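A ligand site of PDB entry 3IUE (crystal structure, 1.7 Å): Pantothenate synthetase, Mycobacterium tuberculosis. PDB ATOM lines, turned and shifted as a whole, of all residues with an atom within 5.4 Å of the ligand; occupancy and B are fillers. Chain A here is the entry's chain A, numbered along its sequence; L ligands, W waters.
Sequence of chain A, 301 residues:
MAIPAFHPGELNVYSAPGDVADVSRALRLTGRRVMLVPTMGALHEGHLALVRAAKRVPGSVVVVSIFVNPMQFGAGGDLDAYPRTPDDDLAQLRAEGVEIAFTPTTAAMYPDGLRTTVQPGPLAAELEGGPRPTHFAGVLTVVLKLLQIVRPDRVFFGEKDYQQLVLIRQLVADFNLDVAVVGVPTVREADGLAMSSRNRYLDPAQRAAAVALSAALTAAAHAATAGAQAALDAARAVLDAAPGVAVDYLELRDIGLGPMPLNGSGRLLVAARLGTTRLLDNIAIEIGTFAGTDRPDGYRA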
ATOM      1  N   PRO A  38      -0.867 -18.720 -10.854  1.00  0.00           N
ATOM      2  CA  PRO A  38      -2.317 -18.865 -10.994  1.00  0.00           C
ATOM      3  C   PRO A  38      -3.016 -18.855  -9.654  1.00  0.00           C
ATOM      4  O   PRO A  38      -2.648 -19.625  -8.745  1.00  0.00           O
ATOM      5  CB  PRO A  38      -2.482 -20.249 -11.637  1.00  0.00           C
ATOM      6  CG  PRO A  38      -1.066 -20.915 -11.602  1.00  0.00           C
ATOM      7  CD  PRO A  38      -0.186 -20.029 -10.771  1.00  0.00           C
ATOM      8  N   THR A  39      -4.015 -17.988  -9.528  1.00  0.00           N
ATOM      9  CA  THR A  39      -4.732 -17.799  -8.264  1.00  0.00           C
ATOM     10  C   THR A  39      -6.266 -17.788  -8.491  1.00  0.00           C
ATOM     11  O   THR A  39      -6.742 -17.703  -9.641  1.00  0.00           O
ATOM     12  CB  THR A  39      -4.360 -16.450  -7.612  1.00  0.00           C
ATOM     13  OG1 THR A  39      -5.111 -15.399  -8.239  1.00  0.00           O
ATOM     14  CG2 THR A  39      -2.841 -16.143  -7.784  1.00  0.00           C
ATOM     15  N   MET A  40      -7.007 -17.903  -7.396  1.00  0.00           N
ATOM     16  CA  MET A  40      -8.468 -17.720  -7.474  1.00  0.00           C
ATOM     17  C   MET A  40      -8.854 -16.362  -6.843  1.00  0.00           C
ATOM     18  O   MET A  40      -9.981 -16.141  -6.401  1.00  0.00           O
ATOM     19  CB  MET A  40      -9.214 -18.915  -6.894  1.00  0.00           C
ATOM     20  CG  MET A  40      -8.883 -20.223  -7.613  1.00  0.00           C
ATOM     21  SD  MET A  40     -10.250 -21.402  -7.663  1.00  0.00           S
ATOM     22  CE  MET A  40     -10.626 -21.491  -5.905  1.00  0.00           C
ATOM     23  N   GLY A  41      -7.877 -15.452  -6.806  1.00  0.00           N
ATOM     24  CA  GLY A  41      -8.124 -14.079  -6.344  1.00  0.00           C
ATOM     25  C   GLY A  41      -8.181 -13.981  -4.824  1.00  0.00           C
ATOM     26  O   GLY A  41      -7.725 -14.882  -4.107  1.00  0.00           O
ATOM     27  N   HIS A  44      -3.596 -12.148  -0.926  1.00  0.00           N
ATOM     28  CA  HIS A  44      -2.966 -11.763   0.322  1.00  0.00           C
ATOM     29  C   HIS A  44      -1.439 -11.831   0.189  1.00  0.00           C
ATOM     30  O   HIS A  44      -0.905 -12.164  -0.878  1.00  0.00           O
ATOM     31  CB  HIS A  44      -3.497 -12.640   1.458  1.00  0.00           C
ATOM     32  CG  HIS A  44      -3.366 -14.113   1.198  1.00  0.00           C
ATOM     33  ND1 HIS A  44      -2.152 -14.747   1.110  1.00  0.00           N
ATOM     34  CD2 HIS A  44      -4.304 -15.073   1.003  1.00  0.00           C
ATOM     35  CE1 HIS A  44      -2.341 -16.030   0.872  1.00  0.00           C
ATOM     36  NE2 HIS A  44      -3.633 -16.255   0.811  1.00  0.00           N
ATOM     37  N   GLY A  46       0.696 -13.836   0.954  1.00  0.00           N
ATOM     38  CA  GLY A  46       1.174 -15.141   0.505  1.00  0.00           C
ATOM     39  C   GLY A  46       1.231 -15.240  -1.015  1.00  0.00           C
ATOM     40  O   GLY A  46       2.228 -15.714  -1.595  1.00  0.00           O
ATOM     41  N   HIS A  47       0.151 -14.786  -1.664  1.00  0.00           N
ATOM     42  CA  HIS A  47       0.151 -14.646  -3.116  1.00  0.00           C
ATOM     43  C   HIS A  47       1.261 -13.689  -3.536  1.00  0.00           C
ATOM     44  O   HIS A  47       1.947 -13.924  -4.532  1.00  0.00           O
ATOM     45  CB  HIS A  47      -1.207 -14.173  -3.650  1.00  0.00           C
ATOM     46  CG  HIS A  47      -2.350 -15.109  -3.386  1.00  0.00           C
ATOM     47  ND1 HIS A  47      -3.272 -14.899  -2.375  1.00  0.00           N
ATOM     48  CD2 HIS A  47      -2.721 -16.264  -3.996  1.00  0.00           C
ATOM     49  CE1 HIS A  47      -4.170 -15.866  -2.398  1.00  0.00           C
ATOM     50  NE2 HIS A  47      -3.857 -16.710  -3.360  1.00  0.00           N
ATOM     51  N   ALA A  49       4.101 -13.104  -2.133  1.00  0.00           N
ATOM     52  CA  ALA A  49       5.354 -13.874  -2.049  1.00  0.00           C
ATOM     53  C   ALA A  49       5.596 -14.676  -3.332  1.00  0.00           C
ATOM     54  O   ALA A  49       6.751 -14.764  -3.805  1.00  0.00           O
ATOM     55  CB  ALA A  49       5.367 -14.794  -0.815  1.00  0.00           C
ATOM     56  N   LEU A  50       4.533 -15.258  -3.896  1.00  0.00           N
ATOM     57  CA  LEU A  50       4.656 -15.984  -5.172  1.00  0.00           C
ATOM     58  C   LEU A  50       5.090 -15.033  -6.289  1.00  0.00           C
ATOM     59  O   LEU A  50       6.031 -15.307  -7.074  1.00  0.00           O
ATOM     60  CB  LEU A  50       3.303 -16.649  -5.522  1.00  0.00           C
ATOM     61  CG  LEU A  50       2.614 -17.555  -4.509  1.00  0.00           C
ATOM     62  CD1 LEU A  50       1.419 -18.210  -5.212  1.00  0.00           C
ATOM     63  CD2 LEU A  50       3.585 -18.634  -3.993  1.00  0.00           C
ATOM     64  N   GLN A  72     -14.055 -26.984  -9.822  1.00  0.00           N
ATOM     65  CA  GLN A  72     -13.489 -27.584  -8.611  1.00  0.00           C
ATOM     66  C   GLN A  72     -14.414 -27.424  -7.363  1.00  0.00           C
ATOM     67  O   GLN A  72     -14.047 -27.790  -6.247  1.00  0.00           O
ATOM     68  CB  GLN A  72     -12.069 -27.071  -8.334  1.00  0.00           C
ATOM     69  CG  GLN A  72     -11.986 -25.622  -7.914  1.00  0.00           C
ATOM     70  CD  GLN A  72     -10.569 -25.102  -7.846  1.00  0.00           C
ATOM     71  OE1 GLN A  72     -10.023 -24.839  -6.742  1.00  0.00           O
ATOM     72  NE2 GLN A  72      -9.927 -24.940  -9.024  1.00  0.00           N
ATOM     73  N   TYR A  82     -17.316 -18.169  -2.180  1.00  0.00           N
ATOM     74  CA  TYR A  82     -15.888 -17.870  -2.340  1.00  0.00           C
ATOM     75  C   TYR A  82     -15.563 -16.375  -2.300  1.00  0.00           C
ATOM     76  O   TYR A  82     -16.243 -15.577  -2.964  1.00  0.00           O
ATOM     77  CB  TYR A  82     -15.311 -18.507  -3.606  1.00  0.00           C
ATOM     78  CG  TYR A  82     -13.810 -18.695  -3.492  1.00  0.00           C
ATOM     79  CD1 TYR A  82     -13.285 -19.797  -2.812  1.00  0.00           C
ATOM     80  CD2 TYR A  82     -12.913 -17.763  -4.023  1.00  0.00           C
ATOM     81  CE1 TYR A  82     -11.894 -19.979  -2.690  1.00  0.00           C
ATOM     82  CE2 TYR A  82     -11.512 -17.931  -3.898  1.00  0.00           C
ATOM     83  CZ  TYR A  82     -11.021 -19.044  -3.217  1.00  0.00           C
ATOM     84  OH  TYR A  82      -9.665 -19.259  -3.087  1.00  0.00           O
ATOM     85  N   HIS A 135     -12.971 -32.789  -6.965  1.00  0.00           N
ATOM     86  CA  HIS A 135     -12.313 -31.505  -6.677  1.00  0.00           C
ATOM     87  C   HIS A 135     -10.982 -31.383  -7.436  1.00  0.00           C
ATOM     88  O   HIS A 135     -10.736 -30.382  -8.113  1.00  0.00           O
ATOM     89  CB  HIS A 135     -12.057 -31.345  -5.158  1.00  0.00           C
ATOM     90  CG  HIS A 135     -11.171 -30.172  -4.829  1.00  0.00           C
ATOM     91  ND1 HIS A 135     -11.626 -28.870  -4.886  1.00  0.00           N
ATOM     92  CD2 HIS A 135      -9.862 -30.103  -4.478  1.00  0.00           C
ATOM     93  CE1 HIS A 135     -10.632 -28.043  -4.580  1.00  0.00           C
ATOM     94  NE2 HIS A 135      -9.554 -28.765  -4.332  1.00  0.00           N
ATOM     95  N   PHE A 157       3.333 -21.846  -7.011  1.00  0.00           N
ATOM     96  CA  PHE A 157       2.277 -22.214  -6.080  1.00  0.00           C
ATOM     97  C   PHE A 157       2.813 -22.114  -4.654  1.00  0.00           C
ATOM     98  O   PHE A 157       3.994 -22.389  -4.404  1.00  0.00           O
ATOM     99  CB  PHE A 157       1.815 -23.663  -6.339  1.00  0.00           C
ATOM    100  CG  PHE A 157       1.105 -23.847  -7.652  1.00  0.00           C
ATOM    101  CD1 PHE A 157      -0.251 -23.526  -7.776  1.00  0.00           C
ATOM    102  CD2 PHE A 157       1.797 -24.299  -8.776  1.00  0.00           C
ATOM    103  CE1 PHE A 157      -0.906 -23.675  -9.000  1.00  0.00           C
ATOM    104  CE2 PHE A 157       1.165 -24.460  -9.975  1.00  0.00           C
ATOM    105  CZ  PHE A 157      -0.192 -24.130 -10.113  1.00  0.00           C
ATOM    106  N   GLY A 158       1.938 -21.744  -3.706  1.00  0.00           N
ATOM    107  CA  GLY A 158       2.282 -21.856  -2.279  1.00  0.00           C
ATOM    108  C   GLY A 158       2.294 -23.301  -1.805  1.00  0.00           C
ATOM    109  O   GLY A 158       1.637 -24.149  -2.389  1.00  0.00           O
ATOM    110  N   GLU A 159       3.051 -23.582  -0.748  1.00  0.00           N
ATOM    111  CA  GLU A 159       3.090 -24.938  -0.169  1.00  0.00           C
ATOM    112  C   GLU A 159       1.918 -25.260   0.762  1.00  0.00           C
ATOM    113  O   GLU A 159       1.766 -26.427   1.155  1.00  0.00           O
ATOM    114  CB  GLU A 159       4.395 -25.160   0.599  1.00  0.00           C
ATOM    115  CG  GLU A 159       5.587 -25.338  -0.328  1.00  0.00           C
ATOM    116  CD  GLU A 159       6.875 -25.610   0.416  1.00  0.00           C
ATOM    117  OE1 GLU A 159       6.883 -25.581   1.668  1.00  0.00           O
ATOM    118  OE2 GLU A 159       7.886 -25.854  -0.263  1.00  0.00           O
ATOM    119  N   LYS A 160       1.088 -24.269   1.113  1.00  0.00           N
ATOM    120  CA  LYS A 160       0.006 -24.517   2.075  1.00  0.00           C
ATOM    121  C   LYS A 160      -0.945 -25.607   1.568  1.00  0.00           C
ATOM    122  O   LYS A 160      -1.316 -26.552   2.287  1.00  0.00           O
ATOM    123  CB  LYS A 160      -0.785 -23.239   2.417  1.00  0.00           C
ATOM    124  CG  LYS A 160      -1.645 -23.445   3.713  1.00  0.00           C
ATOM    125  CD  LYS A 160      -2.979 -22.632   3.743  1.00  0.00           C
ATOM    126  CE  LYS A 160      -4.021 -23.431   2.968  1.00  0.00           C
ATOM    127  NZ  LYS A 160      -5.342 -22.741   2.828  1.00  0.00           N
ATOM    128  N   ASP A 161      -1.332 -25.499   0.305  1.00  0.00           N
ATOM    129  CA  ASP A 161      -2.155 -26.541  -0.286  1.00  0.00           C
ATOM    130  C   ASP A 161      -1.185 -27.555  -0.905  1.00  0.00           C
ATOM    131  O   ASP A 161      -0.986 -27.641  -2.141  1.00  0.00           O
ATOM    132  CB  ASP A 161      -3.120 -25.979  -1.324  1.00  0.00           C
ATOM    133  CG  ASP A 161      -4.115 -25.005  -0.702  1.00  0.00           C
ATOM    134  OD1 ASP A 161      -5.157 -25.449  -0.214  1.00  0.00           O
ATOM    135  OD2 ASP A 161      -3.848 -23.784  -0.693  1.00  0.00           O
ATOM    136  N   GLN A 164      -2.433 -30.304  -3.365  1.00  0.00           N
ATOM    137  CA  GLN A 164      -2.629 -29.714  -4.681  1.00  0.00           C
ATOM    138  C   GLN A 164      -1.286 -29.566  -5.430  1.00  0.00           C
ATOM    139  O   GLN A 164      -1.176 -29.888  -6.602  1.00  0.00           O
ATOM    140  CB  GLN A 164      -3.320 -28.362  -4.537  1.00  0.00           C
ATOM    141  CG  GLN A 164      -3.440 -27.619  -5.847  1.00  0.00           C
ATOM    142  CD  GLN A 164      -4.153 -26.304  -5.677  1.00  0.00           C
ATOM    143  OE1 GLN A 164      -5.348 -26.285  -5.563  1.00  0.00           O
ATOM    144  NE2 GLN A 164      -3.405 -25.208  -5.653  1.00  0.00           N
ATOM    145  N   VAL A 184       6.524 -22.490  -3.170  1.00  0.00           N
ATOM    146  CA  VAL A 184       7.016 -21.394  -2.316  1.00  0.00           C
ATOM    147  C   VAL A 184       6.578 -21.607  -0.864  1.00  0.00           C
ATOM    148  O   VAL A 184       5.392 -21.850  -0.596  1.00  0.00           O
ATOM    149  CB  VAL A 184       6.485 -20.031  -2.832  1.00  0.00           C
ATOM    150  CG1 VAL A 184       6.948 -18.869  -1.940  1.00  0.00           C
ATOM    151  CG2 VAL A 184       6.923 -19.806  -4.263  1.00  0.00           C
ATOM    152  N   PRO A 185       7.526 -21.557   0.098  1.00  0.00           N
ATOM    153  CA  PRO A 185       7.109 -21.874   1.468  1.00  0.00           C
ATOM    154  C   PRO A 185       6.033 -20.915   1.939  1.00  0.00           C
ATOM    155  O   PRO A 185       6.045 -19.706   1.614  1.00  0.00           O
ATOM    156  CB  PRO A 185       8.400 -21.707   2.283  1.00  0.00           C
ATOM    157  CG  PRO A 185       9.537 -21.931   1.246  1.00  0.00           C
ATOM    158  CD  PRO A 185       8.987 -21.296   0.002  1.00  0.00           C
ATOM    159  N   THR A 186       5.102 -21.495   2.699  1.00  0.00           N
ATOM    160  CA  THR A 186       3.920 -20.811   3.231  1.00  0.00           C
ATOM    161  C   THR A 186       4.227 -19.558   4.052  1.00  0.00           C
ATOM    162  O   THR A 186       4.955 -19.632   5.046  1.00  0.00           O
ATOM    163  CB  THR A 186       3.085 -21.807   4.096  1.00  0.00           C
ATOM    164  OG1 THR A 186       2.652 -22.903   3.252  1.00  0.00           O
ATOM    165  CG2 THR A 186       1.856 -21.134   4.699  1.00  0.00           C
ATOM    166  N   VAL A 187       3.664 -18.420   3.645  1.00  0.00           N
ATOM    167  CA  VAL A 187       3.783 -17.159   4.403  1.00  0.00           C
ATOM    168  C   VAL A 187       2.834 -17.232   5.597  1.00  0.00           C
ATOM    169  O   VAL A 187       1.720 -17.761   5.469  1.00  0.00           O
ATOM    170  CB  VAL A 187       3.417 -15.909   3.564  1.00  0.00           C
ATOM    171  CG1 VAL A 187       3.579 -14.640   4.402  1.00  0.00           C
ATOM    172  CG2 VAL A 187       4.281 -15.816   2.297  1.00  0.00           C
ATOM    173  N   MET A 195      -1.211 -18.064   6.147  1.00  0.00           N
ATOM    174  CA  MET A 195      -2.047 -17.112   5.419  1.00  0.00           C
ATOM    175  C   MET A 195      -3.084 -17.859   4.601  1.00  0.00           C
ATOM    176  O   MET A 195      -2.800 -18.928   4.066  1.00  0.00           O
ATOM    177  CB  MET A 195      -1.188 -16.293   4.465  1.00  0.00           C
ATOM    178  CG  MET A 195      -0.125 -15.617   5.187  1.00  0.00           C
ATOM    179  SD  MET A 195      -0.807 -14.067   5.577  1.00  0.00           S
ATOM    180  CE  MET A 195       0.147 -13.210   4.403  1.00  0.00           C
ATOM    181  N   SER A 196      -4.283 -17.303   4.541  1.00  0.00           N
ATOM    182  CA  SER A 196      -5.349 -17.889   3.747  1.00  0.00           C
ATOM    183  C   SER A 196      -6.403 -16.865   3.460  1.00  0.00           C
ATOM    184  O   SER A 196      -6.746 -16.068   4.344  1.00  0.00           O
ATOM    185  CB  SER A 196      -6.016 -19.057   4.513  1.00  0.00           C
ATOM    186  OG  SER A 196      -7.129 -19.560   3.775  1.00  0.00           O
ATOM    187  N   SER A 197      -6.954 -16.925   2.254  1.00  0.00           N
ATOM    188  CA  SER A 197      -8.124 -16.103   1.904  1.00  0.00           C
ATOM    189  C   SER A 197      -9.343 -16.510   2.755  1.00  0.00           C
ATOM    190  O   SER A 197     -10.361 -15.826   2.749  1.00  0.00           O
ATOM    191  CB  SER A 197      -8.456 -16.235   0.414  1.00  0.00           C
ATOM    192  OG  SER A 197      -8.847 -17.567   0.125  1.00  0.00           O
ATOM    193  N   ARG A 198      -9.241 -17.623   3.481  1.00  0.00           N
ATOM    194  CA  ARG A 198     -10.392 -17.998   4.316  1.00  0.00           C
ATOM    195  C   ARG A 198     -10.212 -17.673   5.814  1.00  0.00           C
ATOM    196  O   ARG A 198     -11.116 -17.914   6.621  1.00  0.00           O
ATOM    197  CB  ARG A 198     -10.850 -19.454   4.094  1.00  0.00           C
ATOM    198  CG  ARG A 198     -11.095 -19.819   2.613  1.00  0.00           C
ATOM    199  CD  ARG A 198     -12.223 -20.846   2.377  1.00  0.00           C
ATOM    200  NE  ARG A 198     -12.602 -21.637   3.561  1.00  0.00           N
ATOM    201  CZ  ARG A 198     -13.606 -22.520   3.583  1.00  0.00           C
ATOM    202  NH1 ARG A 198     -14.325 -22.746   2.484  1.00  0.00           N
ATOM    203  NH2 ARG A 198     -13.899 -23.193   4.689  1.00  0.00           N
HETATM  204  C1  LIG L   1      -4.897 -19.745   0.916  1.00  0.00           C
HETATM  205  N1  LIG L   1      -2.525 -19.765  -0.250  1.00  0.00           N
HETATM  206  O1  LIG L   1      -5.134 -18.594   0.489  1.00  0.00           O
HETATM  207  C2  LIG L   1      -3.523 -20.332   0.735  1.00  0.00           C
HETATM  208  C3  LIG L   1       3.615 -18.485  -0.136  1.00  0.00           C
HETATM  209  C4  LIG L   1      -8.110 -24.595  -2.991  1.00  0.00           C
HETATM  210  O2  LIG L   1      -4.762 -20.156  -1.954  1.00  0.00           O
HETATM  211  O3  LIG L   1      -3.883 -20.662  -6.083  1.00  0.00           O
HETATM  212  O4  LIG L   1      -5.348 -18.876  -5.002  1.00  0.00           O
HETATM  213  C5  LIG L   1      -7.831 -22.251  -3.652  1.00  0.00           C
HETATM  214  C6  LIG L   1      -7.000 -21.220  -4.094  1.00  0.00           C
HETATM  215  C7  LIG L   1       0.545 -18.968   1.617  1.00  0.00           C
HETATM  216  C8  LIG L   1      -0.767 -19.377   1.424  1.00  0.00           C
HETATM  217  C9  LIG L   1      -5.920 -23.764  -3.604  1.00  0.00           C
HETATM  218  C10 LIG L   1       0.714 -18.585  -0.739  1.00  0.00           C
HETATM  219  C11 LIG L   1      -1.367 -19.139  -1.983  1.00  0.00           C
HETATM  220  N2  LIG L   1      -5.104 -22.704  -4.020  1.00  0.00           N
HETATM  221  N3  LIG L   1      -3.354 -19.880  -3.691  1.00  0.00           N
HETATM  222  O5  LIG L   1       2.609 -18.159   0.824  1.00  0.00           O
HETATM  223  C12 LIG L   1      -3.630 -19.889  -2.390  1.00  0.00           C
HETATM  224  C13 LIG L   1      -7.291 -23.535  -3.421  1.00  0.00           C
HETATM  225  C14 LIG L   1       1.323 -18.575   0.542  1.00  0.00           C
HETATM  226  C15 LIG L   1      -5.624 -21.467  -4.262  1.00  0.00           C
HETATM  227  C16 LIG L   1      -2.564 -19.619  -1.580  1.00  0.00           C
HETATM  228  C17 LIG L   1      -0.566 -19.013  -0.897  1.00  0.00           C
HETATM  229  C18 LIG L   1      -1.296 -19.411   0.172  1.00  0.00           C
HETATM  230  S1  LIG L   1      -4.552 -20.161  -4.805  1.00  0.00           S
HETATM  231  O6  LIG L   1      -5.686 -20.486   1.545  1.00  0.00           O
HETATM  232  O   HOH W   1      -0.759 -21.305  -4.705  1.00  0.00           O
HETATM  233  O   HOH W   2      -7.008 -24.370  -6.601  1.00  0.00           O
HETATM  234  O   HOH W   3      -6.285 -22.565  -0.584  1.00  0.00           O
HETATM  235  O   HOH W   4      -6.592 -18.168  -1.931  1.00  0.00           O
HETATM  236  O   HOH W   5      -2.193 -23.217  -3.816  1.00  0.00           O
HETATM  237  O   HOH W   6      -6.889 -27.722  -3.940  1.00  0.00           O
HETATM  238  O   HOH W   7      -7.834 -17.596  -4.191  1.00  0.00           O
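NZ of Lys 160 lies within salt-bridge range of OD2 of Asp 161, 3.96 Å away.
N of Lys 160 is in hydrogen-bond range of OG1 of Thr 186, 3.0 Å away.
The backbone NH (N) of Arg 198 is in hydrogen-bond range of the side-chain hydroxyl (OG) of Ser 196, 2.9 Å away.
The backbone NH of Met 195 sits close to the backbone carbonyl oxygen of Val 187, at 3.0 Å.
The side-chain sulfur (SD) of Met 40 lies close to the side-chain amide oxygen (OE1) of Gln 72, 3.6 Å away.
The backbone NH (N) of Gly 41 is in hydrogen-bond range of the side-chain hydroxyl (OG1) of Thr 39 (3.1 Å).
The backbone NH (N) of Val 184 is in hydrogen-bond range of the backbone carbonyl oxygen (O) of Phe 157 (2.8 Å).
O of Val 184 lies within hydrogen-bond range of N of Glu 159, 2.9 Å away.
The side-chain amino group of Lys 160 is in salt-bridge range of an oxygen (O6) of the ligand, at 2.6 Å.
NE2 of His 44 sits at hydrogen-bond distance from O1 of the ligand, at 2.8 Å.
An oxygen (O6) of the ligand lies within hydrogen-bond range of the side-chain hydroxyl (OG) of Ser 196, at 2.8 Å.
The backbone NH (N) of Val 187 is in hydrogen-bond range of an oxygen (O5) of the ligand.
N of Ser 197 sits at hydrogen-bond distance from O1 of the ligand, 3.0 Å away.
The backbone NH (N) of Met 40 sits at hydrogen-bond distance from an oxygen (O4) of the ligand, 3.1 Å away.
NE2 of His 47 sits at hydrogen-bond distance from O4 of the ligand (3.1 Å).
N2 of the ligand is in hydrogen-bond range of NE2 of Gln 164 (3.4 Å).
O of Pro 38 sits close to O3 of the ligand (3.1 Å).
The backbone carbonyl oxygen (O) of Gly 46 lies close to an oxygen (O5) of the ligand (3.5 Å).
CA of Thr 39 touches O4 of the ligand (3.5 Å).
Leu 50 touches the ligand (CD2 to C3, 3.9 Å).
OH of Tyr 82 touches C6 of the ligand, 3.5 Å away.
Gly 158 touches the ligand (CA to C10, 3.9 Å).
Asp 161 touches the ligand.
CG1 of Val 184 touches C3 of the ligand, at 3.8 Å.
Pro 185 touches the ligand.
Thr 186 touches the ligand (CA to O5, 3.8 Å).
Met 195 touches the ligand (O to C8, 3.4 Å).
Hydrophobic or aromatic side chains that line the ligand: Met 40, His 44, His 47, Leu 50, Val 184 and Val 187.
Of the 26 residues printed, 19 come within 4 Å of the ligand.
Along chain A the residues within 4 Å of the ligand span positions 38 to 197.
Water W4 lies within hydrogen-bond range of O2 of the ligand (2.7 Å), OG of Ser 197 (3.1 Å), NE2 of His 47 (3.4 Å) and OH of Tyr 82 (3.5 Å).
Water W5 bridges N2 of the ligand (3.0 Å) and NE2 of Gln 164 (3.0 Å).
Water W3 lies within hydrogen-bond range of OD2 of Asp 161 and O6 of the ligand.
Water W1 bridges the backbone NH (N) of Gly 158 (2.9 Å) and a nitrogen (N3) of the ligand (3.1 Å).
Water W2 lies within hydrogen-bond range of OE1 of Gln 164 (2.7 Å) and OE1 of Gln 72 (3.1 Å).
Water W6 lies within hydrogen-bond range of OE1 of Gln 164 (2.7 Å) and NE2 of His 135 (2.9 Å).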
